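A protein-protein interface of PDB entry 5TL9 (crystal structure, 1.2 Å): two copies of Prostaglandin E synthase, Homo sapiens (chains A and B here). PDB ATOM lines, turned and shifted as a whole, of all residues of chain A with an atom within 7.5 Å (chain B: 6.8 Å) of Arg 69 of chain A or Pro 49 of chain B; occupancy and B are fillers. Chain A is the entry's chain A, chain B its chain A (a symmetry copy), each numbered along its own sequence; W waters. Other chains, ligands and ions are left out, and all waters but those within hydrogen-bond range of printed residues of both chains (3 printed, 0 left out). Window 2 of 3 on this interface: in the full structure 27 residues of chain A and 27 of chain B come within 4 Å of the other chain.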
ATOM      1  N   VAL A  32      16.245 -15.676   3.752  1.00  0.00           N
ATOM      2  CA  VAL A  32      16.186 -16.788   4.703  1.00  0.00           C
ATOM      3  C   VAL A  32      17.518 -16.981   5.435  1.00  0.00           C
ATOM      4  O   VAL A  32      17.522 -17.174   6.648  1.00  0.00           O
ATOM      5  CB  VAL A  32      15.690 -18.092   4.038  1.00  0.00           C
ATOM      6  CG1 VAL A  32      15.787 -19.284   4.985  1.00  0.00           C
ATOM      7  CG2 VAL A  32      14.251 -17.921   3.574  1.00  0.00           C
ATOM      8  N   THR A  36      17.961 -16.502   9.420  1.00  0.00           N
ATOM      9  CA  THR A  36      18.562 -17.583  10.202  1.00  0.00           C
ATOM     10  C   THR A  36      19.624 -17.031  11.160  1.00  0.00           C
ATOM     11  O   THR A  36      19.618 -17.351  12.352  1.00  0.00           O
ATOM     12  CB  THR A  36      19.178 -18.670   9.295  1.00  0.00           C
ATOM     13  OG1 THR A  36      18.183 -19.178   8.401  1.00  0.00           O
ATOM     14  CG2 THR A  36      19.711 -19.823  10.121  1.00  0.00           C
ATOM     15  N   ASP A  64      18.108 -25.053  18.471  1.00  0.00           N
ATOM     16  CA  ASP A  64      16.938 -24.250  18.814  1.00  0.00           C
ATOM     17  C   ASP A  64      15.840 -24.549  17.795  1.00  0.00           C
ATOM     18  O   ASP A  64      16.141 -24.650  16.607  1.00  0.00           O
ATOM     19  CB  ASP A  64      17.301 -22.762  18.817  1.00  0.00           C
ATOM     20  CG  ASP A  64      16.106 -21.860  19.001  1.00  0.00           C
ATOM     21  OD1 ASP A  64      15.476 -21.493  17.986  1.00  0.00           O
ATOM     22  OD2 ASP A  64      15.800 -21.510  20.161  1.00  0.00           O
ATOM     23  N   PRO A  65      14.569 -24.681  18.245  1.00  0.00           N
ATOM     24  CA  PRO A  65      13.502 -25.036  17.291  1.00  0.00           C
ATOM     25  C   PRO A  65      13.290 -24.018  16.165  1.00  0.00           C
ATOM     26  O   PRO A  65      13.016 -24.419  15.029  1.00  0.00           O
ATOM     27  CB  PRO A  65      12.247 -25.139  18.168  1.00  0.00           C
ATOM     28  CG  PRO A  65      12.755 -25.353  19.549  1.00  0.00           C
ATOM     29  CD  PRO A  65      14.066 -24.629  19.632  1.00  0.00           C
ATOM     30  N   ASP A  66      13.413 -22.727  16.466  1.00  0.00           N
ATOM     31  CA  ASP A  66      13.252 -21.692  15.439  1.00  0.00           C
ATOM     32  C   ASP A  66      14.413 -21.679  14.442  1.00  0.00           C
ATOM     33  O   ASP A  66      14.198 -21.479  13.245  1.00  0.00           O
ATOM     34  CB  ASP A  66      13.023 -20.311  16.059  1.00  0.00           C
ATOM     35  CG  ASP A  66      11.723 -20.226  16.838  1.00  0.00           C
ATOM     36  OD1 ASP A  66      10.702 -20.774  16.373  1.00  0.00           O
ATOM     37  OD2 ASP A  66      11.726 -19.604  17.917  1.00  0.00           O
ATOM     38  N   VAL A  67      15.634 -21.905  14.931  1.00  0.00           N
ATOM     39  CA  VAL A  67      16.793 -22.049  14.041  1.00  0.00           C
ATOM     40  C   VAL A  67      16.589 -23.264  13.123  1.00  0.00           C
ATOM     41  O   VAL A  67      16.759 -23.160  11.909  1.00  0.00           O
ATOM     42  CB  VAL A  67      18.131 -22.154  14.817  1.00  0.00           C
ATOM     43  CG1 VAL A  67      19.286 -22.403  13.857  1.00  0.00           C
ATOM     44  CG2 VAL A  67      18.402 -20.888  15.623  1.00  0.00           C
ATOM     45  N   GLU A  68      16.193 -24.396  13.700  1.00  0.00           N
ATOM     46  CA  GLU A  68      15.939 -25.609  12.923  1.00  0.00           C
ATOM     47  C   GLU A  68      14.855 -25.388  11.864  1.00  0.00           C
ATOM     48  O   GLU A  68      14.995 -25.856  10.734  1.00  0.00           O
ATOM     49  CB  GLU A  68      15.586 -26.784  13.840  1.00  0.00           C
ATOM     50  CG  GLU A  68      16.756 -27.294  14.677  1.00  0.00           C
ATOM     51  CD  GLU A  68      16.358 -28.273  15.774  1.00  0.00           C
ATOM     52  OE1 GLU A  68      15.164 -28.373  16.117  1.00  0.00           O
ATOM     53  OE2 GLU A  68      17.255 -28.946  16.317  1.00  0.00           O
ATOM     54  N   ARG A  69      13.798 -24.657  12.223  1.00  0.00           N
ATOM     55  CA  ARG A  69      12.734 -24.292  11.285  1.00  0.00           C
ATOM     56  C   ARG A  69      13.276 -23.465  10.111  1.00  0.00           C
ATOM     57  O   ARG A  69      12.957 -23.744   8.948  1.00  0.00           O
ATOM     58  CB  ARG A  69      11.626 -23.537  12.020  1.00  0.00           C
ATOM     59  CG  ARG A  69      10.468 -23.093  11.136  1.00  0.00           C
ATOM     60  CD  ARG A  69       9.357 -22.447  11.949  1.00  0.00           C
ATOM     61  NE  ARG A  69       8.653 -23.424  12.786  1.00  0.00           N
ATOM     62  CZ  ARG A  69       7.579 -24.120  12.411  1.00  0.00           C
ATOM     63  NH1 ARG A  69       7.041 -23.948  11.208  1.00  0.00           N
ATOM     64  NH2 ARG A  69       7.030 -24.989  13.254  1.00  0.00           N
ATOM     65  N   CYS A  70      14.107 -22.466  10.418  1.00  0.00           N
ATOM     66  CA  CYS A  70      14.766 -21.669   9.380  1.00  0.00           C
ATOM     67  C   CYS A  70      15.586 -22.539   8.431  1.00  0.00           C
ATOM     68  O   CYS A  70      15.504 -22.367   7.207  1.00  0.00           O
ATOM     69  CB  CYS A  70      15.660 -20.590   9.993  1.00  0.00           C
ATOM     70  SG  CYS A  70      14.772 -19.221  10.762  1.00  0.00           S
ATOM     71  N   LEU A  71      16.352 -23.471   8.992  1.00  0.00           N
ATOM     72  CA  LEU A  71      17.150 -24.389   8.189  1.00  0.00           C
ATOM     73  C   LEU A  71      16.278 -25.291   7.320  1.00  0.00           C
ATOM     74  O   LEU A  71      16.635 -25.563   6.178  1.00  0.00           O
ATOM     75  CB  LEU A  71      18.104 -25.207   9.062  1.00  0.00           C
ATOM     76  CG  LEU A  71      19.282 -24.431   9.665  1.00  0.00           C
ATOM     77  CD1 LEU A  71      19.891 -25.195  10.829  1.00  0.00           C
ATOM     78  CD2 LEU A  71      20.336 -24.130   8.610  1.00  0.00           C
ATOM     79  N   ARG A  72      15.129 -25.724   7.842  1.00  0.00           N
ATOM     80  CA  ARG A  72      14.193 -26.537   7.050  1.00  0.00           C
ATOM     81  C   ARG A  72      13.645 -25.767   5.855  1.00  0.00           C
ATOM     82  O   ARG A  72      13.566 -26.309   4.750  1.00  0.00           O
ATOM     83  CB  ARG A  72      13.038 -27.073   7.893  1.00  0.00           C
ATOM     84  CG  ARG A  72      13.451 -28.150   8.875  1.00  0.00           C
ATOM     85  CD  ARG A  72      12.260 -28.936   9.401  1.00  0.00           C
ATOM     86  NE  ARG A  72      11.339 -28.158  10.237  1.00  0.00           N
ATOM     87  CZ  ARG A  72      11.533 -27.872  11.523  1.00  0.00           C
ATOM     88  NH1 ARG A  72      12.640 -28.270  12.142  1.00  0.00           N
ATOM     89  NH2 ARG A  72      10.618 -27.173  12.187  1.00  0.00           N
ATOM     90  N   ALA A  73      13.282 -24.503   6.068  1.00  0.00           N
ATOM     91  CA  ALA A  73      12.793 -23.664   4.979  1.00  0.00           C
ATOM     92  C   ALA A  73      13.875 -23.476   3.917  1.00  0.00           C
ATOM     93  O   ALA A  73      13.610 -23.603   2.719  1.00  0.00           O
ATOM     94  CB  ALA A  73      12.316 -22.324   5.509  1.00  0.00           C
ATOM     95  N   HIS A  74      15.099 -23.202   4.367  1.00  0.00           N
ATOM     96  CA  HIS A  74      16.232 -23.025   3.471  1.00  0.00           C
ATOM     97  C   HIS A  74      16.538 -24.311   2.698  1.00  0.00           C
ATOM     98  O   HIS A  74      16.779 -24.268   1.485  1.00  0.00           O
ATOM     99  CB  HIS A  74      17.460 -22.560   4.260  1.00  0.00           C
ATOM    100  CG  HIS A  74      18.448 -21.781   3.449  1.00  0.00           C
ATOM    101  ND1 HIS A  74      19.456 -21.044   4.032  1.00  0.00           N
ATOM    102  CD2 HIS A  74      18.581 -21.610   2.109  1.00  0.00           C
ATOM    103  CE1 HIS A  74      20.173 -20.462   3.087  1.00  0.00           C
ATOM    104  NE2 HIS A  74      19.665 -20.791   1.912  1.00  0.00           N
ATOM    105  N   ARG A  75      16.506 -25.452   3.387  1.00  0.00           N
ATOM    106  CA  ARG A  75      16.712 -26.745   2.733  1.00  0.00           C
ATOM    107  C   ARG A  75      15.623 -27.010   1.694  1.00  0.00           C
ATOM    108  O   ARG A  75      15.917 -27.414   0.565  1.00  0.00           O
ATOM    109  CB  ARG A  75      16.787 -27.879   3.765  1.00  0.00           C
ATOM    110  CG  ARG A  75      16.890 -29.270   3.145  1.00  0.00           C
ATOM    111  CD  ARG A  75      16.834 -30.432   4.150  1.00  0.00           C
ATOM    112  NE  ARG A  75      15.803 -30.344   5.209  1.00  0.00           N
ATOM    113  CZ  ARG A  75      14.480 -30.356   5.031  1.00  0.00           C
ATOM    114  NH1 ARG A  75      13.688 -30.256   6.090  1.00  0.00           N
ATOM    115  NH2 ARG A  75      13.944 -30.446   3.816  1.00  0.00           N
ATOM    116  N   ALA A 118       4.545 -19.199   4.974  1.00  0.00           N
ATOM    117  CA  ALA A 118       3.816 -20.241   5.698  1.00  0.00           C
ATOM    118  C   ALA A 118       4.712 -21.051   6.630  1.00  0.00           C
ATOM    119  O   ALA A 118       4.267 -21.472   7.706  1.00  0.00           O
ATOM    120  CB  ALA A 118       3.086 -21.158   4.728  1.00  0.00           C
ATOM    121  N   TYR A 119       5.970 -21.259   6.221  1.00  0.00           N
ATOM    122  CA  TYR A 119       6.921 -22.038   7.014  1.00  0.00           C
ATOM    123  C   TYR A 119       7.422 -21.245   8.214  1.00  0.00           C
ATOM    124  O   TYR A 119       7.265 -21.674   9.362  1.00  0.00           O
ATOM    125  CB  TYR A 119       8.129 -22.520   6.178  1.00  0.00           C
ATOM    126  CG  TYR A 119       8.611 -23.911   6.558  1.00  0.00           C
ATOM    127  CD1 TYR A 119       8.284 -24.471   7.799  1.00  0.00           C
ATOM    128  CD2 TYR A 119       9.385 -24.676   5.676  1.00  0.00           C
ATOM    129  CE1 TYR A 119       8.689 -25.747   8.147  1.00  0.00           C
ATOM    130  CE2 TYR A 119       9.803 -25.960   6.016  1.00  0.00           C
ATOM    131  CZ  TYR A 119       9.444 -26.492   7.253  1.00  0.00           C
ATOM    132  OH  TYR A 119       9.805 -27.764   7.631  1.00  0.00           O
ATOM    133  N   LEU A 120       8.023 -20.090   7.946  1.00  0.00           N
ATOM    134  CA  LEU A 120       8.582 -19.266   9.011  1.00  0.00           C
ATOM    135  C   LEU A 120       7.502 -18.650   9.892  1.00  0.00           C
ATOM    136  O   LEU A 120       7.736 -18.424  11.075  1.00  0.00           O
ATOM    137  CB  LEU A 120       9.517 -18.195   8.442  1.00  0.00           C
ATOM    138  CG  LEU A 120      10.706 -18.692   7.602  1.00  0.00           C
ATOM    139  CD1 LEU A 120      11.597 -17.523   7.215  1.00  0.00           C
ATOM    140  CD2 LEU A 120      11.520 -19.776   8.300  1.00  0.00           C
ATOM    141  N   GLY A 121       6.329 -18.407   9.305  1.00  0.00           N
ATOM    142  CA  GLY A 121       5.174 -17.880  10.028  1.00  0.00           C
ATOM    143  C   GLY A 121       4.392 -18.904  10.824  1.00  0.00           C
ATOM    144  O   GLY A 121       3.462 -18.534  11.537  1.00  0.00           O
ATOM    145  N   LYS A 122       4.759 -20.185  10.704  1.00  0.00           N
ATOM    146  CA  LYS A 122       4.119 -21.293  11.441  1.00  0.00           C
ATOM    147  C   LYS A 122       2.602 -21.332  11.194  1.00  0.00           C
ATOM    148  O   LYS A 122       1.811 -21.526  12.122  1.00  0.00           O
ATOM    149  CB  LYS A 122       4.447 -21.235  12.952  1.00  0.00           C
ATOM    150  CG  LYS A 122       5.924 -21.092  13.277  1.00  0.00           C
ATOM    151  CD  LYS A 122       6.179 -20.940  14.767  1.00  0.00           C
ATOM    152  CE  LYS A 122       7.637 -20.595  15.019  1.00  0.00           C
ATOM    153  NZ  LYS A 122       7.945 -20.422  16.465  1.00  0.00           N
ATOM    154  N   LEU A 123       2.203 -21.137   9.939  1.00  0.00           N
ATOM    155  CA  LEU A 123       0.788 -21.122   9.586  1.00  0.00           C
ATOM    156  C   LEU A 123       0.216 -22.528   9.659  1.00  0.00           C
ATOM    157  O   LEU A 123       0.944 -23.511   9.491  1.00  0.00           O
ATOM    158  CB  LEU A 123       0.564 -20.481   8.211  1.00  0.00           C
ATOM    159  CG  LEU A 123       0.963 -19.005   8.036  1.00  0.00           C
ATOM    160  CD1 LEU A 123       0.533 -18.520   6.663  1.00  0.00           C
ATOM    161  CD2 LEU A 123       0.405 -18.086   9.119  1.00  0.00           C
ATOM    162  N   ALA A 125      -1.463 -26.109   9.086  1.00  0.00           N
ATOM    163  CA  ALA A 125      -1.488 -27.063   7.987  1.00  0.00           C
ATOM    164  C   ALA A 125      -2.910 -27.108   7.388  1.00  0.00           C
ATOM    165  O   ALA A 125      -3.880 -26.903   8.126  1.00  0.00           O
ATOM    166  CB  ALA A 125      -1.050 -28.431   8.481  1.00  0.00           C
ATOM    167  N   ARG A 128       1.214 -24.526   4.143  1.00  0.00           N
ATOM    168  CA  ARG A 128       2.555 -24.713   3.580  1.00  0.00           C
ATOM    169  C   ARG A 128       2.594 -25.822   2.522  1.00  0.00           C
ATOM    170  O   ARG A 128       3.158 -25.629   1.440  1.00  0.00           O
ATOM    171  CB  ARG A 128       3.582 -24.998   4.678  1.00  0.00           C
ATOM    172  CG  ARG A 128       5.023 -24.992   4.186  1.00  0.00           C
ATOM    173  CD  ARG A 128       5.955 -25.691   5.154  1.00  0.00           C
ATOM    174  NE  ARG A 128       5.793 -27.145   5.152  1.00  0.00           N
ATOM    175  CZ  ARG A 128       5.216 -27.867   6.115  1.00  0.00           C
ATOM    176  NH1 ARG A 128       4.712 -27.298   7.214  1.00  0.00           N
ATOM    177  NH2 ARG A 128       5.150 -29.185   5.975  1.00  0.00           N
ATOM    178  N   PHE B  46       6.569 -36.200  11.605  1.00  0.00           N
ATOM    179  CA  PHE B  46       6.510 -34.872  11.012  1.00  0.00           C
ATOM    180  C   PHE B  46       7.548 -33.968  11.640  1.00  0.00           C
ATOM    181  O   PHE B  46       7.891 -34.122  12.813  1.00  0.00           O
ATOM    182  CB  PHE B  46       5.091 -34.309  11.140  1.00  0.00           C
ATOM    183  CG  PHE B  46       4.049 -35.236  10.595  1.00  0.00           C
ATOM    184  CD1 PHE B  46       3.837 -35.334   9.216  1.00  0.00           C
ATOM    185  CD2 PHE B  46       3.314 -36.067  11.452  1.00  0.00           C
ATOM    186  CE1 PHE B  46       2.905 -36.226   8.702  1.00  0.00           C
ATOM    187  CE2 PHE B  46       2.384 -36.962  10.941  1.00  0.00           C
ATOM    188  CZ  PHE B  46       2.177 -37.037   9.566  1.00  0.00           C
ATOM    189  N   ALA B  47       8.053 -33.034  10.843  1.00  0.00           N
ATOM    190  CA  ALA B  47       9.105 -32.130  11.292  1.00  0.00           C
ATOM    191  C   ALA B  47       8.567 -30.922  12.053  1.00  0.00           C
ATOM    192  O   ALA B  47       9.318 -30.245  12.757  1.00  0.00           O
ATOM    193  CB  ALA B  47       9.932 -31.677  10.104  1.00  0.00           C
ATOM    194  N   ASN B  48       7.266 -30.664  11.914  1.00  0.00           N
ATOM    195  CA  ASN B  48       6.652 -29.432  12.402  1.00  0.00           C
ATOM    196  C   ASN B  48       5.446 -29.723  13.266  1.00  0.00           C
ATOM    197  O   ASN B  48       4.634 -30.580  12.900  1.00  0.00           O
ATOM    198  CB  ASN B  48       6.234 -28.558  11.224  1.00  0.00           C
ATOM    199  CG  ASN B  48       7.384 -28.283  10.285  1.00  0.00           C
ATOM    200  OD1 ASN B  48       8.357 -27.635  10.665  1.00  0.00           O
ATOM    201  ND2 ASN B  48       7.288 -28.791   9.059  1.00  0.00           N
ATOM    202  N   PRO B  49       5.300 -28.995  14.398  1.00  0.00           N
ATOM    203  CA  PRO B  49       4.130 -29.210  15.262  1.00  0.00           C
ATOM    204  C   PRO B  49       2.801 -28.975  14.541  1.00  0.00           C
ATOM    205  O   PRO B  49       1.838 -29.706  14.794  1.00  0.00           O
ATOM    206  CB  PRO B  49       4.325 -28.195  16.391  1.00  0.00           C
ATOM    207  CG  PRO B  49       5.788 -27.937  16.422  1.00  0.00           C
ATOM    208  CD  PRO B  49       6.247 -28.034  14.998  1.00  0.00           C
ATOM    209  N   GLU B  50       2.749 -27.993  13.637  1.00  0.00           N
ATOM    210  CA  GLU B  50       1.515 -27.717  12.889  1.00  0.00           C
ATOM    211  C   GLU B  50       1.108 -28.888  11.980  1.00  0.00           C
ATOM    212  O   GLU B  50      -0.083 -29.150  11.796  1.00  0.00           O
ATOM    213  CB  GLU B  50       1.571 -26.376  12.128  1.00  0.00           C
ATOM    214  CG  GLU B  50       2.594 -26.268  10.993  1.00  0.00           C
ATOM    215  CD  GLU B  50       3.978 -25.804  11.427  1.00  0.00           C
ATOM    216  OE1 GLU B  50       4.372 -25.980  12.602  1.00  0.00           O
ATOM    217  OE2 GLU B  50       4.693 -25.266  10.564  1.00  0.00           O
ATOM    218  N   ASP B  51       2.098 -29.605  11.443  1.00  0.00           N
ATOM    219  CA  ASP B  51       1.843 -30.802  10.639  1.00  0.00           C
ATOM    220  C   ASP B  51       1.314 -31.925  11.525  1.00  0.00           C
ATOM    221  O   ASP B  51       0.293 -32.546  11.210  1.00  0.00           O
ATOM    222  CB  ASP B  51       3.120 -31.291   9.932  1.00  0.00           C
ATOM    223  CG  ASP B  51       3.728 -30.264   8.982  1.00  0.00           C
ATOM    224  OD1 ASP B  51       3.085 -29.249   8.634  1.00  0.00           O
ATOM    225  OD2 ASP B  51       4.886 -30.492   8.569  1.00  0.00           O
ATOM    226  N   ALA B  52       2.012 -32.171  12.637  1.00  0.00           N
ATOM    227  CA  ALA B  52       1.656 -33.233  13.576  1.00  0.00           C
ATOM    228  C   ALA B  52       0.231 -33.094  14.113  1.00  0.00           C
ATOM    229  O   ALA B  52      -0.503 -34.080  14.176  1.00  0.00           O
ATOM    230  CB  ALA B  52       2.653 -33.279  14.718  1.00  0.00           C
ATOM    231  N   LEU B  53      -0.160 -31.868  14.460  1.00  0.00           N
ATOM    232  CA  LEU B  53      -1.500 -31.610  14.995  1.00  0.00           C
ATOM    233  C   LEU B  53      -2.615 -31.928  14.001  1.00  0.00           C
ATOM    234  O   LEU B  53      -3.698 -32.343  14.409  1.00  0.00           O
ATOM    235  CB  LEU B  53      -1.626 -30.174  15.521  1.00  0.00           C
ATOM    236  CG  LEU B  53      -0.877 -29.809  16.811  1.00  0.00           C
ATOM    237  CD1 LEU B  53      -0.913 -28.309  17.052  1.00  0.00           C
ATOM    238  CD2 LEU B  53      -1.404 -30.549  18.032  1.00  0.00           C
ATOM    239  N   ARG B  54      -2.349 -31.735  12.709  1.00  0.00           N
ATOM    240  CA  ARG B  54      -3.301 -32.104  11.658  1.00  0.00           C
ATOM    241  C   ARG B  54      -3.372 -33.622  11.448  1.00  0.00           C
ATOM    242  O   ARG B  54      -4.430 -34.153  11.100  1.00  0.00           O
ATOM    243  CB  ARG B  54      -2.974 -31.381  10.347  1.00  0.00           C
ATOM    244  CG  ARG B  54      -3.830 -31.806   9.162  1.00  0.00           C
ATOM    245  CD  ARG B  54      -3.709 -30.840   8.005  1.00  0.00           C
ATOM    246  NE  ARG B  54      -4.330 -31.354   6.788  1.00  0.00           N
ATOM    247  CZ  ARG B  54      -5.624 -31.238   6.486  1.00  0.00           C
ATOM    248  NH1 ARG B  54      -6.474 -30.637   7.316  1.00  0.00           N
ATOM    249  NH2 ARG B  54      -6.070 -31.737   5.346  1.00  0.00           N
ATOM    250  N   GLY B  57      -1.852 -35.708  16.228  1.00  0.00           N
ATOM    251  CA  GLY B  57      -1.497 -35.146  17.526  1.00  0.00           C
ATOM    252  C   GLY B  57      -0.041 -34.738  17.662  1.00  0.00           C
ATOM    253  O   GLY B  57       0.795 -35.121  16.834  1.00  0.00           O
ATOM    254  N   PRO B  58       0.284 -33.979  18.726  1.00  0.00           N
ATOM    255  CA  PRO B  58       1.616 -33.386  18.910  1.00  0.00           C
ATOM    256  C   PRO B  58       2.737 -34.414  19.077  1.00  0.00           C
ATOM    257  O   PRO B  58       3.894 -34.103  18.783  1.00  0.00           O
ATOM    258  CB  PRO B  58       1.459 -32.552  20.187  1.00  0.00           C
ATOM    259  CG  PRO B  58       0.338 -33.193  20.928  1.00  0.00           C
ATOM    260  CD  PRO B  58      -0.601 -33.699  19.877  1.00  0.00           C
ATOM    261  N   CSO B  61       5.182 -35.133  16.070  1.00  0.00           N
ATOM    262  CA  CSO B  61       6.299 -34.248  15.714  1.00  0.00           C
ATOM    263  CB  CSO B  61       6.140 -32.818  16.241  1.00  0.00           C
ATOM    264  SG  CSO B  61       7.390 -31.752  15.579  1.00  0.00           S
ATOM    265  C   CSO B  61       7.510 -34.926  16.294  1.00  0.00           C
ATOM    266  O   CSO B  61       7.811 -34.782  17.481  1.00  0.00           O
ATOM    267  OD  CSO B  61       8.612 -31.666  16.808  1.00  0.00           O
HETATM  268  O   HOH W   1      11.830 -31.212  13.640  1.00  0.00           O
HETATM  269  O   HOH W   2      -1.953 -27.134  11.788  1.00  0.00           O
HETATM  270  O   HOH W   3       4.157 -24.402   8.043  1.00  0.00           O
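The side-chain amide oxygen (OD1) of Asn 48 of chain B is in hydrogen-bond range of the guanidinium group (NH2) of Arg 72 of chain A, 2.8 Å away.
The guanidinium group (NH1) of Arg 69 of chain A lies within salt-bridge range of the side-chain carboxylate (OE2) of Glu 50 of chain B, at 2.8 Å.
The side-chain carboxylate (OE2) of Glu 50 of chain B lies within salt-bridge range of the guanidinium group (NH1) of Arg 128 of chain A.
The guanidinium group (NH1) of Arg 128 of chain A lies within salt-bridge range of the side-chain carboxylate (OD1) of Asp 51 of chain B.
The side-chain amide nitrogen (ND2) of Asn 48 of chain B is in hydrogen-bond range of the side-chain hydroxyl (OH) of Tyr 119 of chain A, at 3.1 Å.
The backbone carbonyl oxygen (O) of Ala 47 of chain B lies within hydrogen-bond range of the guanidinium group (NH2) of Arg 72 of chain A.
NE of Arg 72 of chain A is in hydrogen-bond range of OH of Tyr 119 of chain A.
The backbone NH (N) of Leu 123 of chain A is in hydrogen-bond range of the backbone carbonyl oxygen (O) of Ala 118 of chain A (3.1 Å).
The guanidinium group of Arg 69 of chain A lies within hydrogen-bond range of the backbone carbonyl oxygen of Tyr 119 of chain A (2.9 Å).
ND2 of Asn 48 of chain B sits at hydrogen-bond distance from OD2 of Asp 51 of chain B, at 3.0 Å.
Asn 48 of chain B touches Arg 69 of chain A (OD1 to NH2, 3.9 Å).
Pro 49 of chain B touches Arg 69 of chain A (CD to NH2, 3.6 Å).
Glu 50 of chain B touches Leu 123 of chain A.
Ala 125 of chain A touches Glu 50 of chain B (CB to O, 3.5 Å).
Arg 54 of chain B touches Ala 125 of chain A.
NH1 of Arg 128 of chain A touches ND2 of Asn 48 of chain B, 3.5 Å away.
Printed residues of chain B within 4 Å of Arg 72 of chain A: Ala 47 and Asn 48.
Of the printed residues of chain A, Pro 49 of chain B touches Arg 69 (3.6 Å).
Printed residues of chain A within 4 Å of Glu 50 of chain B: Arg 69 (2.8 Å), Leu 123 (3.5 Å), Ala 125 (3.5 Å) and Arg 128 (3.9 Å).
The nearest residue of chain B that does not touch Arg 69 of chain A is Ala 47 of chain B (5.8 Å).
Hydrophobic or aromatic side chains of chain A that line the printed part of chain B: Tyr 119 and Ala 125.
Among the printed residues, Asp or Glu carboxylates within 4 Å of a Lys or Arg side-chain nitrogen of the other chain: Arg 69 of chain A with Glu 50 of chain B (2.8 Å), Arg 128 of chain A with Glu 50 of chain B (3.9 Å) and Arg 128 of chain A with Asp 51 of chain B (2.9 Å).
No position is printed for both chains.
Water W3 lies within hydrogen-bond range of the side-chain carboxylate of Glu 50 of chain B, the backbone carbonyl oxygen of Ala 118 of chain A and the guanidinium group of Arg 128 of chain A.
Water W2 lies within hydrogen-bond range of O of Glu 50 of chain B (2.7 Å) and N of Ala 125 of chain A (2.9 Å).
Water W1 lies within hydrogen-bond range of O of Ala 47 of chain B (2.8 Å) and NH1 of Arg 72 of chain A (3.4 Å).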
